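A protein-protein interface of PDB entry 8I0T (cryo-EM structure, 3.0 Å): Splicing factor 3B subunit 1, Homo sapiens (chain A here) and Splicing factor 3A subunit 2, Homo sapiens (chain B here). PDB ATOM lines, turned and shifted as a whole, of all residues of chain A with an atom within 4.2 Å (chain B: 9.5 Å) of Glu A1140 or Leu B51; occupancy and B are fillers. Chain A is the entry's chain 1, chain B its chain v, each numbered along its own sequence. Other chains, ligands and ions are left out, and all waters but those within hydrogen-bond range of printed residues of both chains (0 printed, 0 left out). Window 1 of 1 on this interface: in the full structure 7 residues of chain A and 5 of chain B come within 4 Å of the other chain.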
ATOM      1  N   LYS A1102      -6.420   6.577  13.318  1.00  0.00           N
ATOM      2  CA  LYS A1102      -4.997   6.241  13.522  1.00  0.00           C
ATOM      3  C   LYS A1102      -4.040   6.919  12.544  1.00  0.00           C
ATOM      4  O   LYS A1102      -2.854   6.898  12.826  1.00  0.00           O
ATOM      5  CB  LYS A1102      -4.771   4.742  13.421  1.00  0.00           C
ATOM      6  CG  LYS A1102      -4.084   4.181  14.604  1.00  0.00           C
ATOM      7  CD  LYS A1102      -4.634   2.832  14.877  1.00  0.00           C
ATOM      8  CE  LYS A1102      -4.297   2.389  16.263  1.00  0.00           C
ATOM      9  NZ  LYS A1102      -4.899   1.064  16.508  1.00  0.00           N
ATOM     10  N   VAL A1138      -6.952   3.208  23.595  1.00  0.00           N
ATOM     11  CA  VAL A1138      -5.764   2.845  22.833  1.00  0.00           C
ATOM     12  C   VAL A1138      -4.710   3.895  23.132  1.00  0.00           C
ATOM     13  O   VAL A1138      -4.996   5.092  23.051  1.00  0.00           O
ATOM     14  CB  VAL A1138      -6.056   2.729  21.335  1.00  0.00           C
ATOM     15  CG1 VAL A1138      -6.954   3.774  20.945  1.00  0.00           C
ATOM     16  CG2 VAL A1138      -4.795   2.875  20.551  1.00  0.00           C
ATOM     17  N   PRO A1139      -3.504   3.509  23.460  1.00  0.00           N
ATOM     18  CA  PRO A1139      -2.605   4.430  24.154  1.00  0.00           C
ATOM     19  C   PRO A1139      -1.999   5.504  23.280  1.00  0.00           C
ATOM     20  O   PRO A1139      -0.949   6.031  23.642  1.00  0.00           O
ATOM     21  CB  PRO A1139      -1.518   3.499  24.695  1.00  0.00           C
ATOM     22  CG  PRO A1139      -1.500   2.387  23.738  1.00  0.00           C
ATOM     23  CD  PRO A1139      -2.937   2.155  23.405  1.00  0.00           C
ATOM     24  N   GLU A1140      -2.554   5.803  22.119  1.00  0.00           N
ATOM     25  CA  GLU A1140      -1.902   6.754  21.238  1.00  0.00           C
ATOM     26  C   GLU A1140      -2.542   8.134  21.283  1.00  0.00           C
ATOM     27  O   GLU A1140      -3.740   8.290  21.544  1.00  0.00           O
ATOM     28  CB  GLU A1140      -1.887   6.238  19.811  1.00  0.00           C
ATOM     29  CG  GLU A1140      -1.205   4.921  19.669  1.00  0.00           C
ATOM     30  CD  GLU A1140      -1.728   4.150  18.495  1.00  0.00           C
ATOM     31  OE1 GLU A1140      -2.337   4.784  17.611  1.00  0.00           O
ATOM     32  OE2 GLU A1140      -1.533   2.919  18.450  1.00  0.00           O
ATOM     33  N   LEU A1141      -1.728   9.136  20.977  1.00  0.00           N
ATOM     34  CA  LEU A1141      -2.140  10.508  21.194  1.00  0.00           C
ATOM     35  C   LEU A1141      -3.185  10.912  20.187  1.00  0.00           C
ATOM     36  O   LEU A1141      -4.361  11.067  20.526  1.00  0.00           O
ATOM     37  CB  LEU A1141      -0.931  11.421  21.072  1.00  0.00           C
ATOM     38  CG  LEU A1141      -1.119  12.832  21.582  1.00  0.00           C
ATOM     39  CD1 LEU A1141      -1.156  12.818  23.087  1.00  0.00           C
ATOM     40  CD2 LEU A1141      -0.007  13.700  21.060  1.00  0.00           C
ATOM     41  N   ASN A1142      -2.794  10.955  18.920  1.00  0.00           N
ATOM     42  CA  ASN A1142      -3.693  11.390  17.867  1.00  0.00           C
ATOM     43  C   ASN A1142      -5.061  10.748  17.991  1.00  0.00           C
ATOM     44  O   ASN A1142      -6.067  11.395  17.707  1.00  0.00           O
ATOM     45  CB  ASN A1142      -3.079  11.076  16.510  1.00  0.00           C
ATOM     46  CG  ASN A1142      -1.973  12.029  16.144  1.00  0.00           C
ATOM     47  OD1 ASN A1142      -1.938  12.570  15.043  1.00  0.00           O
ATOM     48  ND2 ASN A1142      -1.069  12.255  17.075  1.00  0.00           N
ATOM     49  N   VAL A1143      -5.141   9.528  18.510  1.00  0.00           N
ATOM     50  CA  VAL A1143      -6.451   8.904  18.590  1.00  0.00           C
ATOM     51  C   VAL A1143      -7.196   9.308  19.845  1.00  0.00           C
ATOM     52  O   VAL A1143      -8.414   9.505  19.800  1.00  0.00           O
ATOM     53  CB  VAL A1143      -6.350   7.382  18.478  1.00  0.00           C
ATOM     54  CG1 VAL A1143      -5.003   6.946  18.811  1.00  0.00           C
ATOM     55  CG2 VAL A1143      -7.320   6.756  19.400  1.00  0.00           C
ATOM     56  N   GLN A1144      -6.531   9.438  20.987  1.00  0.00           N
ATOM     57  CA  GLN A1144      -7.280   9.938  22.131  1.00  0.00           C
ATOM     58  C   GLN A1144      -7.804  11.339  21.868  1.00  0.00           C
ATOM     59  O   GLN A1144      -8.946  11.673  22.222  1.00  0.00           O
ATOM     60  CB  GLN A1144      -6.417   9.907  23.363  1.00  0.00           C
ATOM     61  CG  GLN A1144      -6.184   8.535  23.826  1.00  0.00           C
ATOM     62  CD  GLN A1144      -5.161   8.492  24.876  1.00  0.00           C
ATOM     63  OE1 GLN A1144      -4.095   9.055  24.719  1.00  0.00           O
ATOM     64  NE2 GLN A1144      -5.469   7.845  25.978  1.00  0.00           N
ATOM     65  N   ARG A1180      -3.373  15.102  30.481  1.00  0.00           N
ATOM     66  CA  ARG A1180      -2.624  14.235  29.603  1.00  0.00           C
ATOM     67  C   ARG A1180      -1.709  15.016  28.661  1.00  0.00           C
ATOM     68  O   ARG A1180      -0.655  14.495  28.282  1.00  0.00           O
ATOM     69  CB  ARG A1180      -3.579  13.336  28.809  1.00  0.00           C
ATOM     70  N   ARG B  24       2.555   5.186   7.915  1.00  0.00           N
ATOM     71  CA  ARG B  24       2.170   4.621   9.202  1.00  0.00           C
ATOM     72  C   ARG B  24       2.964   3.364   9.502  1.00  0.00           C
ATOM     73  O   ARG B  24       3.427   3.161  10.630  1.00  0.00           O
ATOM     74  CB  ARG B  24       0.675   4.321   9.209  1.00  0.00           C
ATOM     75  CG  ARG B  24       0.128   3.882  10.543  1.00  0.00           C
ATOM     76  CD  ARG B  24      -1.145   3.075  10.377  1.00  0.00           C
ATOM     77  NE  ARG B  24      -2.238   3.874   9.837  1.00  0.00           N
ATOM     78  CZ  ARG B  24      -3.487   3.435   9.695  1.00  0.00           C
ATOM     79  NH1 ARG B  24      -4.427   4.230   9.198  1.00  0.00           N
ATOM     80  NH2 ARG B  24      -3.797   2.196  10.048  1.00  0.00           N
ATOM     81  N   ARG B  27       6.619   3.975  10.184  1.00  0.00           N
ATOM     82  CA  ARG B  27       6.687   4.344  11.587  1.00  0.00           C
ATOM     83  C   ARG B  27       6.672   3.124  12.486  1.00  0.00           C
ATOM     84  O   ARG B  27       7.545   2.969  13.350  1.00  0.00           O
ATOM     85  CB  ARG B  27       5.535   5.268  11.937  1.00  0.00           C
ATOM     86  CG  ARG B  27       5.399   5.551  13.408  1.00  0.00           C
ATOM     87  CD  ARG B  27       4.162   6.388  13.661  1.00  0.00           C
ATOM     88  NE  ARG B  27       3.898   7.347  12.587  1.00  0.00           N
ATOM     89  CZ  ARG B  27       4.706   8.343  12.229  1.00  0.00           C
ATOM     90  NH1 ARG B  27       5.839   8.566  12.878  1.00  0.00           N
ATOM     91  NH2 ARG B  27       4.365   9.138  11.227  1.00  0.00           N
ATOM     92  N   GLU B  28       5.671   2.265  12.328  1.00  0.00           N
ATOM     93  CA  GLU B  28       5.558   1.114  13.214  1.00  0.00           C
ATOM     94  C   GLU B  28       6.788   0.217  13.142  1.00  0.00           C
ATOM     95  O   GLU B  28       7.288  -0.251  14.176  1.00  0.00           O
ATOM     96  CB  GLU B  28       4.305   0.326  12.886  1.00  0.00           C
ATOM     97  CG  GLU B  28       3.276   0.429  13.963  1.00  0.00           C
ATOM     98  CD  GLU B  28       1.892   0.186  13.444  1.00  0.00           C
ATOM     99  OE1 GLU B  28       1.740  -0.702  12.583  1.00  0.00           O
ATOM    100  OE2 GLU B  28       0.954   0.875  13.892  1.00  0.00           O
ATOM    101  N   ARG B  31       9.462   1.600  15.099  1.00  0.00           N
ATOM    102  CA  ARG B  31       9.254   1.405  16.527  1.00  0.00           C
ATOM    103  C   ARG B  31       9.699   0.019  16.957  1.00  0.00           C
ATOM    104  O   ARG B  31      10.286  -0.151  18.028  1.00  0.00           O
ATOM    105  CB  ARG B  31       7.792   1.632  16.871  1.00  0.00           C
ATOM    106  CG  ARG B  31       7.359   0.988  18.150  1.00  0.00           C
ATOM    107  CD  ARG B  31       5.880   1.164  18.305  1.00  0.00           C
ATOM    108  NE  ARG B  31       5.457   2.436  17.730  1.00  0.00           N
ATOM    109  CZ  ARG B  31       4.307   2.616  17.093  1.00  0.00           C
ATOM    110  NH1 ARG B  31       3.463   1.608  16.967  1.00  0.00           N
ATOM    111  NH2 ARG B  31       3.993   3.804  16.597  1.00  0.00           N
ATOM    112  N   MET B  47      10.809   3.845  29.305  1.00  0.00           N
ATOM    113  CA  MET B  47       9.368   3.751  29.442  1.00  0.00           C
ATOM    114  C   MET B  47       8.705   4.137  28.131  1.00  0.00           C
ATOM    115  O   MET B  47       9.189   5.004  27.407  1.00  0.00           O
ATOM    116  CB  MET B  47       8.862   4.654  30.554  1.00  0.00           C
ATOM    117  CG  MET B  47       7.402   4.513  30.848  1.00  0.00           C
ATOM    118  SD  MET B  47       7.161   5.053  32.530  1.00  0.00           S
ATOM    119  CE  MET B  47       8.228   3.864  33.322  1.00  0.00           C
ATOM    120  N   LYS B  48       7.597   3.482  27.830  1.00  0.00           N
ATOM    121  CA  LYS B  48       6.680   3.947  26.807  1.00  0.00           C
ATOM    122  C   LYS B  48       5.397   4.357  27.508  1.00  0.00           C
ATOM    123  O   LYS B  48       4.752   3.530  28.159  1.00  0.00           O
ATOM    124  CB  LYS B  48       6.416   2.871  25.762  1.00  0.00           C
ATOM    125  CG  LYS B  48       6.499   3.389  24.350  1.00  0.00           C
ATOM    126  CD  LYS B  48       6.123   2.328  23.330  1.00  0.00           C
ATOM    127  CE  LYS B  48       5.695   2.959  22.011  1.00  0.00           C
ATOM    128  NZ  LYS B  48       4.567   2.228  21.379  1.00  0.00           N
ATOM    129  N   ASN B  49       5.035   5.628  27.388  1.00  0.00           N
ATOM    130  CA  ASN B  49       3.986   6.187  28.216  1.00  0.00           C
ATOM    131  C   ASN B  49       2.636   5.917  27.578  1.00  0.00           C
ATOM    132  O   ASN B  49       2.536   5.555  26.406  1.00  0.00           O
ATOM    133  CB  ASN B  49       4.212   7.678  28.414  1.00  0.00           C
ATOM    134  CG  ASN B  49       4.665   8.341  27.161  1.00  0.00           C
ATOM    135  OD1 ASN B  49       4.637   7.737  26.100  1.00  0.00           O
ATOM    136  ND2 ASN B  49       5.091   9.583  27.261  1.00  0.00           N
ATOM    137  N   HIS B  50       1.590   6.123  28.347  1.00  0.00           N
ATOM    138  CA  HIS B  50       0.231   5.910  27.891  1.00  0.00           C
ATOM    139  C   HIS B  50      -0.153   6.797  26.690  1.00  0.00           C
ATOM    140  O   HIS B  50      -1.302   6.734  26.272  1.00  0.00           O
ATOM    141  CB  HIS B  50      -0.731   6.165  29.036  1.00  0.00           C
ATOM    142  CG  HIS B  50      -1.003   7.612  29.254  1.00  0.00           C
ATOM    143  ND1 HIS B  50      -0.012   8.565  29.213  1.00  0.00           N
ATOM    144  CD2 HIS B  50      -2.158   8.279  29.468  1.00  0.00           C
ATOM    145  CE1 HIS B  50      -0.541   9.755  29.432  1.00  0.00           C
ATOM    146  NE2 HIS B  50      -1.843   9.610  29.580  1.00  0.00           N
ATOM    147  N   LEU B  51       0.720   7.642  26.151  1.00  0.00           N
ATOM    148  CA  LEU B  51       0.447   8.366  24.922  1.00  0.00           C
ATOM    149  C   LEU B  51       1.331   7.923  23.770  1.00  0.00           C
ATOM    150  O   LEU B  51       1.280   8.527  22.699  1.00  0.00           O
ATOM    151  CB  LEU B  51       0.616   9.864  25.130  1.00  0.00           C
ATOM    152  CG  LEU B  51      -0.097  10.476  26.320  1.00  0.00           C
ATOM    153  CD1 LEU B  51       0.032  11.990  26.285  1.00  0.00           C
ATOM    154  CD2 LEU B  51      -1.539  10.042  26.318  1.00  0.00           C
ATOM    155  N   GLY B  52       2.149   6.897  23.963  1.00  0.00           N
ATOM    156  CA  GLY B  52       2.963   6.400  22.872  1.00  0.00           C
ATOM    157  C   GLY B  52       4.224   7.177  22.583  1.00  0.00           C
ATOM    158  O   GLY B  52       4.769   7.066  21.486  1.00  0.00           O
ATOM    159  N   SER B  53       4.708   7.959  23.529  1.00  0.00           N
ATOM    160  CA  SER B  53       6.013   8.584  23.449  1.00  0.00           C
ATOM    161  C   SER B  53       7.016   7.702  24.190  1.00  0.00           C
ATOM    162  O   SER B  53       6.718   6.567  24.568  1.00  0.00           O
ATOM    163  CB  SER B  53       5.960   9.995  24.023  1.00  0.00           C
ATOM    164  OG  SER B  53       6.459  10.023  25.345  1.00  0.00           O
ATOM    165  N   TYR B  54       8.216   8.220  24.398  1.00  0.00           N
ATOM    166  CA  TYR B  54       9.212   7.499  25.165  1.00  0.00           C
ATOM    167  C   TYR B  54       9.730   8.369  26.294  1.00  0.00           C
ATOM    168  O   TYR B  54       9.759   9.596  26.195  1.00  0.00           O
ATOM    169  CB  TYR B  54      10.369   7.073  24.286  1.00  0.00           C
ATOM    170  CG  TYR B  54       9.930   6.444  23.007  1.00  0.00           C
ATOM    171  CD1 TYR B  54       9.133   5.324  23.019  1.00  0.00           C
ATOM    172  CD2 TYR B  54      10.325   6.958  21.785  1.00  0.00           C
ATOM    173  CE1 TYR B  54       8.734   4.733  21.859  1.00  0.00           C
ATOM    174  CE2 TYR B  54       9.929   6.373  20.618  1.00  0.00           C
ATOM    175  CZ  TYR B  54       9.129   5.256  20.663  1.00  0.00           C
ATOM    176  OH  TYR B  54       8.710   4.652  19.509  1.00  0.00           O
ATOM    177  N   GLU B  55      10.157   7.719  27.366  1.00  0.00           N
ATOM    178  CA  GLU B  55      10.731   8.410  28.507  1.00  0.00           C
ATOM    179  C   GLU B  55      12.128   7.889  28.780  1.00  0.00           C
ATOM    180  O   GLU B  55      12.496   6.786  28.380  1.00  0.00           O
ATOM    181  CB  GLU B  55       9.932   8.224  29.798  1.00  0.00           C
ATOM    182  CG  GLU B  55       8.499   8.648  29.769  1.00  0.00           C
ATOM    183  CD  GLU B  55       7.967   8.877  31.174  1.00  0.00           C
ATOM    184  OE1 GLU B  55       7.274   9.891  31.402  1.00  0.00           O
ATOM    185  OE2 GLU B  55       8.259   8.049  32.066  1.00  0.00           O
ATOM    186  N   LEU B  62      11.169  13.371  27.811  1.00  0.00           N
ATOM    187  CA  LEU B  62      10.081  12.876  26.997  1.00  0.00           C
ATOM    188  C   LEU B  62      10.427  13.081  25.537  1.00  0.00           C
ATOM    189  O   LEU B  62      10.846  14.168  25.136  1.00  0.00           O
ATOM    190  CB  LEU B  62       8.788  13.592  27.325  1.00  0.00           C
ATOM    191  CG  LEU B  62       8.477  13.641  28.811  1.00  0.00           C
ATOM    192  CD1 LEU B  62       7.255  14.484  29.031  1.00  0.00           C
ATOM    193  CD2 LEU B  62       8.255  12.244  29.321  1.00  0.00           C
ATOM    194  N   HIS B  63      10.240  12.032  24.749  1.00  0.00           N
ATOM    195  CA  HIS B  63      10.595  12.054  23.344  1.00  0.00           C
ATOM    196  C   HIS B  63       9.423  11.611  22.500  1.00  0.00           C
ATOM    197  O   HIS B  63       8.712  10.670  22.854  1.00  0.00           O
ATOM    198  CB  HIS B  63      11.764  11.135  23.054  1.00  0.00           C
ATOM    199  CG  HIS B  63      12.955  11.404  23.902  1.00  0.00           C
ATOM    200  ND1 HIS B  63      14.064  12.061  23.426  1.00  0.00           N
ATOM    201  CD2 HIS B  63      13.207  11.123  25.199  1.00  0.00           C
ATOM    202  CE1 HIS B  63      14.952  12.169  24.393  1.00  0.00           C
ATOM    203  NE2 HIS B  63      14.458  11.604  25.478  1.00  0.00           N
ATOM    204  N   ASN B  64       9.251  12.279  21.372  1.00  0.00           N
ATOM    205  CA  ASN B  64       8.377  11.742  20.350  1.00  0.00           C
ATOM    206  C   ASN B  64       8.886  10.400  19.856  1.00  0.00           C
ATOM    207  O   ASN B  64       8.211   9.381  20.006  1.00  0.00           O
ATOM    208  CB  ASN B  64       8.264  12.726  19.193  1.00  0.00           C
ATOM    209  CG  ASN B  64       8.283  14.147  19.655  1.00  0.00           C
ATOM    210  OD1 ASN B  64       7.700  14.476  20.690  1.00  0.00           O
ATOM    211  ND2 ASN B  64       8.963  15.007  18.905  1.00  0.00           N
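The backbone carbonyl oxygen (O) of Pro A1139 is in hydrogen-bond range of the backbone NH (N) of Gly B52, 3.2 Å away. O of His B50 lies close to O of Pro A1139 (2.7 Å). The backbone carbonyl oxygen (O) of Pro A1139 lies close to the backbone NH (N) of Leu B51 (3.4 Å).
O of Glu A1140 sits close to OE1 of Gln A1144, 3.3 Å away. The side-chain amide oxygen (OD1) of Asn B49 lies within hydrogen-bond range of the backbone NH (N) of Gly B52 (3.4 Å).
Glu A1140 touches Leu B51. Leu A1141 touches Leu B51 (CD1 to CD1, 3.5 Å). Gln A1144 touches His B50 (OE1 to O, 3.9 Å). Gln A1144 touches Leu B51. Arg A1180 touches Leu B51 (O to CD1, 3.3 Å).
Lys A1102 touches none of the printed residues of chain B. No residue of chain B comes within 4 Å of Val A1138. Of chain B, only His B50, Leu B51 and Gly B52 come within 4 Å of Pro A1139. Of chain B, only Leu B51 (3.9 Å) comes within 4 Å of Glu A1140. Of the printed residues of chain B, Leu A1141 touches Leu B51. Of the printed residues of chain B, Gln A1144 touches His B50 and Leu B51. Of the printed residues of chain B, Arg A1180 touches Leu B51 (3.3 Å). Of the printed residues of chain A, Leu B51 touches Pro A1139 (3.0 Å), Glu A1140 (3.9 Å), Leu A1141 (3.5 Å), Gln A1144 (3.2 Å) and Arg A1180 (3.3 Å). Printed residues of chain A within 4 Å of Gly B52: Pro A1139 (3.2 Å).
Printed residues of chain B that touch a printed residue of chain A: His B50, Leu B51 and Gly B52. Hydrophobic or aromatic side chains of chain B within 4 Å of the printed part of chain A: Leu B51. Along chain B the printed residues that touch a printed residue of chain A span positions 50 to 52. Among the printed residues, no Asp or Glu carboxylate lies within 4 Å of a Lys or Arg side-chain nitrogen of the other chain.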
